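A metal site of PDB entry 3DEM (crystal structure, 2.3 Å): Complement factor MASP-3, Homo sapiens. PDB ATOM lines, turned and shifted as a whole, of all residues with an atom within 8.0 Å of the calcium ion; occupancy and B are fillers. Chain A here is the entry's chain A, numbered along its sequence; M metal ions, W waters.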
ATOM      1  N   TYR A  21      16.722 -23.903 -17.212  1.00  0.00           N
ATOM      2  CA  TYR A  21      16.460 -23.306 -18.510  1.00  0.00           C
ATOM      3  C   TYR A  21      15.085 -22.651 -18.589  1.00  0.00           C
ATOM      4  O   TYR A  21      14.152 -23.052 -17.878  1.00  0.00           O
ATOM      5  CB  TYR A  21      16.639 -24.320 -19.646  1.00  0.00           C
ATOM      6  CG  TYR A  21      15.827 -25.587 -19.531  1.00  0.00           C
ATOM      7  CD1 TYR A  21      14.475 -25.615 -19.874  1.00  0.00           C
ATOM      8  CD2 TYR A  21      16.416 -26.784 -19.125  1.00  0.00           C
ATOM      9  CE1 TYR A  21      13.735 -26.775 -19.784  1.00  0.00           C
ATOM     10  CE2 TYR A  21      15.676 -27.954 -19.031  1.00  0.00           C
ATOM     11  CZ  TYR A  21      14.332 -27.946 -19.366  1.00  0.00           C
ATOM     12  OH  TYR A  21      13.599 -29.100 -19.285  1.00  0.00           O
ATOM     13  N   PRO A  22      14.948 -21.619 -19.447  1.00  0.00           N
ATOM     14  CA  PRO A  22      13.674 -20.930 -19.598  1.00  0.00           C
ATOM     15  C   PRO A  22      12.689 -21.769 -20.409  1.00  0.00           C
ATOM     16  O   PRO A  22      13.093 -22.695 -21.113  1.00  0.00           O
ATOM     17  CB  PRO A  22      14.055 -19.659 -20.366  1.00  0.00           C
ATOM     18  CG  PRO A  22      15.275 -20.053 -21.143  1.00  0.00           C
ATOM     19  CD  PRO A  22      16.007 -21.052 -20.303  1.00  0.00           C
ATOM     20  N   SER A  23      11.396 -21.465 -20.282  1.00  0.00           N
ATOM     21  CA  SER A  23      10.383 -22.167 -21.042  1.00  0.00           C
ATOM     22  C   SER A  23      10.266 -21.566 -22.430  1.00  0.00           C
ATOM     23  O   SER A  23      10.782 -20.478 -22.693  1.00  0.00           O
ATOM     24  CB  SER A  23       9.032 -22.122 -20.314  1.00  0.00           C
ATOM     25  OG  SER A  23       8.581 -20.795 -20.184  1.00  0.00           O
ATOM     26  N   ASP A  24       9.581 -22.285 -23.329  1.00  0.00           N
ATOM     27  CA  ASP A  24       9.376 -21.838 -24.705  1.00  0.00           C
ATOM     28  C   ASP A  24      10.656 -21.364 -25.370  1.00  0.00           C
ATOM     29  O   ASP A  24      10.698 -20.283 -25.956  1.00  0.00           O
ATOM     30  CB  ASP A  24       8.304 -20.749 -24.780  1.00  0.00           C
ATOM     31  CG  ASP A  24       8.022 -20.309 -26.207  1.00  0.00           C
ATOM     32  OD1 ASP A  24       8.057 -21.167 -27.118  1.00  0.00           O
ATOM     33  OD2 ASP A  24       7.754 -19.102 -26.430  1.00  0.00           O
ATOM     34  N   LEU A  48      16.725 -32.924 -17.843  1.00  0.00           N
ATOM     35  CA  LEU A  48      15.552 -32.455 -18.582  1.00  0.00           C
ATOM     36  C   LEU A  48      14.266 -33.083 -18.092  1.00  0.00           C
ATOM     37  O   LEU A  48      14.279 -34.075 -17.358  1.00  0.00           O
ATOM     38  CB  LEU A  48      15.714 -32.727 -20.075  1.00  0.00           C
ATOM     39  CG  LEU A  48      16.237 -31.594 -20.969  1.00  0.00           C
ATOM     40  CD1 LEU A  48      17.728 -31.377 -20.765  1.00  0.00           C
ATOM     41  CD2 LEU A  48      15.938 -31.898 -22.434  1.00  0.00           C
ATOM     42  N   GLU A  49      13.138 -32.499 -18.503  1.00  0.00           N
ATOM     43  CA  GLU A  49      11.830 -33.097 -18.269  1.00  0.00           C
ATOM     44  C   GLU A  49      11.708 -34.395 -19.078  1.00  0.00           C
ATOM     45  O   GLU A  49      12.169 -34.470 -20.211  1.00  0.00           O
ATOM     46  CB  GLU A  49      10.735 -32.112 -18.698  1.00  0.00           C
ATOM     47  CG  GLU A  49       9.314 -32.569 -18.383  1.00  0.00           C
ATOM     48  CD  GLU A  49       8.265 -31.657 -18.996  1.00  0.00           C
ATOM     49  OE1 GLU A  49       8.641 -30.701 -19.718  1.00  0.00           O
ATOM     50  OE2 GLU A  49       7.062 -31.884 -18.767  1.00  0.00           O
ATOM     51  N   SER A  50      11.087 -35.416 -18.510  1.00  0.00           N
ATOM     52  CA  SER A  50      10.886 -36.661 -19.243  1.00  0.00           C
ATOM     53  C   SER A  50       9.514 -36.704 -19.930  1.00  0.00           C
ATOM     54  O   SER A  50       8.526 -36.222 -19.381  1.00  0.00           O
ATOM     55  CB  SER A  50      11.047 -37.871 -18.315  1.00  0.00           C
ATOM     56  OG  SER A  50      11.066 -39.099 -19.044  1.00  0.00           O
ATOM     57  N   TYR A  56       7.975 -33.374 -25.207  1.00  0.00           N
ATOM     58  CA  TYR A  56       7.930 -32.067 -24.524  1.00  0.00           C
ATOM     59  C   TYR A  56       9.272 -31.354 -24.599  1.00  0.00           C
ATOM     60  O   TYR A  56       9.514 -30.565 -25.509  1.00  0.00           O
ATOM     61  CB  TYR A  56       7.438 -32.226 -23.082  1.00  0.00           C
ATOM     62  CG  TYR A  56       6.040 -32.805 -22.970  1.00  0.00           C
ATOM     63  CD1 TYR A  56       5.597 -33.414 -21.799  1.00  0.00           C
ATOM     64  CD2 TYR A  56       5.166 -32.757 -24.057  1.00  0.00           C
ATOM     65  CE1 TYR A  56       4.314 -33.939 -21.706  1.00  0.00           C
ATOM     66  CE2 TYR A  56       3.883 -33.296 -23.973  1.00  0.00           C
ATOM     67  CZ  TYR A  56       3.468 -33.882 -22.796  1.00  0.00           C
ATOM     68  OH  TYR A  56       2.185 -34.402 -22.720  1.00  0.00           O
ATOM     69  N   ASP A  57      10.160 -31.624 -23.638  1.00  0.00           N
ATOM     70  CA  ASP A  57      11.498 -31.065 -23.668  1.00  0.00           C
ATOM     71  C   ASP A  57      12.458 -32.097 -24.254  1.00  0.00           C
ATOM     72  O   ASP A  57      12.329 -33.292 -23.996  1.00  0.00           O
ATOM     73  CB  ASP A  57      11.949 -30.640 -22.271  1.00  0.00           C
ATOM     74  CG  ASP A  57      11.082 -29.555 -21.681  1.00  0.00           C
ATOM     75  OD1 ASP A  57      10.156 -29.076 -22.382  1.00  0.00           O
ATOM     76  OD2 ASP A  57      11.311 -29.162 -20.518  1.00  0.00           O
ATOM     77  N   TYR A  58      13.429 -31.640 -25.038  1.00  0.00           N
ATOM     78  CA  TYR A  58      14.355 -32.581 -25.667  1.00  0.00           C
ATOM     79  C   TYR A  58      15.641 -31.977 -26.193  1.00  0.00           C
ATOM     80  O   TYR A  58      15.735 -30.775 -26.462  1.00  0.00           O
ATOM     81  CB  TYR A  58      13.653 -33.343 -26.786  1.00  0.00           C
ATOM     82  CG  TYR A  58      13.166 -32.479 -27.933  1.00  0.00           C
ATOM     83  CD1 TYR A  58      14.028 -32.060 -28.932  1.00  0.00           C
ATOM     84  CD2 TYR A  58      11.829 -32.102 -28.009  1.00  0.00           C
ATOM     85  CE1 TYR A  58      13.587 -31.276 -29.979  1.00  0.00           C
ATOM     86  CE2 TYR A  58      11.382 -31.321 -29.063  1.00  0.00           C
ATOM     87  CZ  TYR A  58      12.264 -30.918 -30.048  1.00  0.00           C
ATOM     88  OH  TYR A  58      11.816 -30.141 -31.085  1.00  0.00           O
ATOM     89  N   PHE A  99      17.990 -27.981 -28.863  1.00  0.00           N
ATOM     90  CA  PHE A  99      17.388 -28.057 -27.545  1.00  0.00           C
ATOM     91  C   PHE A  99      16.041 -27.354 -27.581  1.00  0.00           C
ATOM     92  O   PHE A  99      15.946 -26.192 -27.965  1.00  0.00           O
ATOM     93  CB  PHE A  99      18.288 -27.408 -26.486  1.00  0.00           C
ATOM     94  CG  PHE A  99      17.585 -27.150 -25.170  1.00  0.00           C
ATOM     95  CD1 PHE A  99      17.346 -28.183 -24.280  1.00  0.00           C
ATOM     96  CD2 PHE A  99      17.172 -25.875 -24.838  1.00  0.00           C
ATOM     97  CE1 PHE A  99      16.695 -27.951 -23.083  1.00  0.00           C
ATOM     98  CE2 PHE A  99      16.520 -25.628 -23.631  1.00  0.00           C
ATOM     99  CZ  PHE A  99      16.289 -26.678 -22.757  1.00  0.00           C
ATOM    100  N   ARG A 100      14.990 -28.071 -27.197  1.00  0.00           N
ATOM    101  CA  ARG A 100      13.668 -27.474 -27.146  1.00  0.00           C
ATOM    102  C   ARG A 100      13.064 -27.576 -25.757  1.00  0.00           C
ATOM    103  O   ARG A 100      13.148 -28.624 -25.106  1.00  0.00           O
ATOM    104  CB  ARG A 100      12.717 -28.123 -28.153  1.00  0.00           C
ATOM    105  CG  ARG A 100      11.379 -27.400 -28.249  1.00  0.00           C
ATOM    106  CD  ARG A 100      10.220 -28.329 -27.944  1.00  0.00           C
ATOM    107  NE  ARG A 100       8.942 -27.625 -27.919  1.00  0.00           N
ATOM    108  CZ  ARG A 100       7.783 -28.208 -27.665  1.00  0.00           C
ATOM    109  NH1 ARG A 100       7.737 -29.513 -27.409  1.00  0.00           N
ATOM    110  NH2 ARG A 100       6.661 -27.502 -27.653  1.00  0.00           N
ATOM    111  N   SER A 101      12.448 -26.493 -25.323  1.00  0.00           N
ATOM    112  CA  SER A 101      11.757 -26.425 -24.055  1.00  0.00           C
ATOM    113  C   SER A 101      10.342 -25.960 -24.349  1.00  0.00           C
ATOM    114  O   SER A 101      10.143 -24.919 -24.968  1.00  0.00           O
ATOM    115  CB  SER A 101      12.481 -25.425 -23.150  1.00  0.00           C
ATOM    116  OG  SER A 101      11.876 -25.335 -21.875  1.00  0.00           O
ATOM    117  N   ASP A 102       9.339 -26.737 -23.948  1.00  0.00           N
ATOM    118  CA  ASP A 102       7.964 -26.319 -24.223  1.00  0.00           C
ATOM    119  C   ASP A 102       7.486 -25.228 -23.266  1.00  0.00           C
ATOM    120  O   ASP A 102       8.301 -24.597 -22.588  1.00  0.00           O
ATOM    121  CB  ASP A 102       6.993 -27.520 -24.280  1.00  0.00           C
ATOM    122  CG  ASP A 102       6.926 -28.286 -22.967  1.00  0.00           C
ATOM    123  OD1 ASP A 102       7.654 -27.945 -22.018  1.00  0.00           O
ATOM    124  OD2 ASP A 102       6.133 -29.253 -22.907  1.00  0.00           O
ATOM    125  N   PHE A 103       6.179 -25.006 -23.213  1.00  0.00           N
ATOM    126  CA  PHE A 103       5.619 -23.919 -22.407  1.00  0.00           C
ATOM    127  C   PHE A 103       5.527 -24.279 -20.933  1.00  0.00           C
ATOM    128  O   PHE A 103       5.373 -23.409 -20.083  1.00  0.00           O
ATOM    129  CB  PHE A 103       4.228 -23.535 -22.934  1.00  0.00           C
ATOM    130  CG  PHE A 103       4.230 -22.971 -24.329  1.00  0.00           C
ATOM    131  CD1 PHE A 103       4.291 -23.800 -25.440  1.00  0.00           C
ATOM    132  CD2 PHE A 103       4.177 -21.587 -24.526  1.00  0.00           C
ATOM    133  CE1 PHE A 103       4.298 -23.278 -26.720  1.00  0.00           C
ATOM    134  CE2 PHE A 103       4.183 -21.055 -25.810  1.00  0.00           C
ATOM    135  CZ  PHE A 103       4.236 -21.901 -26.907  1.00  0.00           C
ATOM    136  N   SER A 104       5.643 -25.568 -20.628  1.00  0.00           N
ATOM    137  CA  SER A 104       5.410 -26.047 -19.277  1.00  0.00           C
ATOM    138  C   SER A 104       6.705 -26.403 -18.543  1.00  0.00           C
ATOM    139  O   SER A 104       7.178 -27.537 -18.618  1.00  0.00           O
ATOM    140  CB  SER A 104       4.487 -27.270 -19.302  1.00  0.00           C
ATOM    141  OG  SER A 104       4.107 -27.651 -17.984  1.00  0.00           O
ATOM    142  N   ASN A 105       7.277 -25.430 -17.827  1.00  0.00           N
ATOM    143  CA  ASN A 105       8.437 -25.689 -16.988  1.00  0.00           C
ATOM    144  C   ASN A 105       8.146 -25.500 -15.495  1.00  0.00           C
ATOM    145  O   ASN A 105       8.829 -24.732 -14.804  1.00  0.00           O
ATOM    146  CB  ASN A 105       9.632 -24.819 -17.413  1.00  0.00           C
ATOM    147  CG  ASN A 105      10.976 -25.526 -17.194  1.00  0.00           C
ATOM    148  OD1 ASN A 105      11.025 -26.738 -17.026  1.00  0.00           O
ATOM    149  ND2 ASN A 105      12.048 -24.755 -17.219  1.00  0.00           N
ATOM    150  N   GLU A 106       7.114 -26.198 -15.005  1.00  0.00           N
ATOM    151  CA  GLU A 106       6.780 -26.251 -13.586  1.00  0.00           C
ATOM    152  C   GLU A 106       8.016 -26.589 -12.753  1.00  0.00           C
ATOM    153  O   GLU A 106       8.507 -25.752 -11.978  1.00  0.00           O
ATOM    154  CB  GLU A 106       5.691 -27.286 -13.329  1.00  0.00           C
ATOM    155  CG  GLU A 106       4.380 -27.053 -14.077  1.00  0.00           C
ATOM    156  CD  GLU A 106       3.394 -26.187 -13.314  1.00  0.00           C
ATOM    157  OE1 GLU A 106       3.821 -25.167 -12.732  1.00  0.00           O
ATOM    158  OE2 GLU A 106       2.193 -26.530 -13.298  1.00  0.00           O
ATOM    159  N   GLU A 107       8.511 -27.818 -12.905  1.00  0.00           N
ATOM    160  CA  GLU A 107       9.765 -28.238 -12.282  1.00  0.00           C
ATOM    161  C   GLU A 107      10.928 -27.499 -12.938  1.00  0.00           C
ATOM    162  O   GLU A 107      10.859 -27.185 -14.123  1.00  0.00           O
ATOM    163  CB  GLU A 107       9.994 -29.744 -12.445  1.00  0.00           C
ATOM    164  CG  GLU A 107       8.902 -30.628 -11.883  1.00  0.00           C
ATOM    165  CD  GLU A 107       9.285 -32.095 -11.937  1.00  0.00           C
ATOM    166  OE1 GLU A 107      10.471 -32.405 -11.700  1.00  0.00           O
ATOM    167  OE2 GLU A 107       8.408 -32.941 -12.206  1.00  0.00           O
ATOM    168  N   PHE A 109      14.340 -27.768 -14.261  1.00  0.00           N
ATOM    169  CA  PHE A 109      15.414 -28.601 -14.770  1.00  0.00           C
ATOM    170  C   PHE A 109      16.589 -27.749 -15.242  1.00  0.00           C
ATOM    171  O   PHE A 109      16.405 -26.714 -15.875  1.00  0.00           O
ATOM    172  CB  PHE A 109      14.873 -29.491 -15.905  1.00  0.00           C
ATOM    173  CG  PHE A 109      13.755 -30.392 -15.473  1.00  0.00           C
ATOM    174  CD1 PHE A 109      12.435 -30.084 -15.750  1.00  0.00           C
ATOM    175  CD2 PHE A 109      14.035 -31.564 -14.771  1.00  0.00           C
ATOM    176  CE1 PHE A 109      11.411 -30.915 -15.352  1.00  0.00           C
ATOM    177  CE2 PHE A 109      13.002 -32.401 -14.363  1.00  0.00           C
ATOM    178  CZ  PHE A 109      11.690 -32.077 -14.653  1.00  0.00           C
HETATM  179 CA    CA M   1       8.941 -28.345 -20.265  1.00  0.00          CA
HETATM  180  O   HOH W   1       9.598 -25.917 -20.910  1.00  0.00           O
HETATM  181  O   HOH W   2       9.689 -28.287 -18.136  1.00  0.00           O
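O of Asp 102 is in hydrogen-bond range of N of Asp 24 (2.7 Å). OD2 of Asp 57 sits close to OH of Tyr 21, at 2.6 Å.
Of the 20 residues printed, 4 come within 4 Å of the calcium ion.
The calcium ion is bound by the side-chain carboxylate (OD1) of Asp 102 (2.2 Å), water W2 (2.3 Å), the side-chain carboxylate (OE1) of Glu 49 (2.4 Å), the side-chain carboxylate (OD2) of Asp 57 (2.5 Å), the backbone carbonyl oxygen (O) of Ser 104 (2.5 Å), the side-chain carboxylate (OD1) of Asp 57 (2.5 Å) and water W1 (2.6 Å). The calcium ion has seven donor atoms within binding distance.
Water W1 lies within hydrogen-bond range of O of Asp 102 (2.5 Å) and OG of Ser 101 (2.5 Å).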
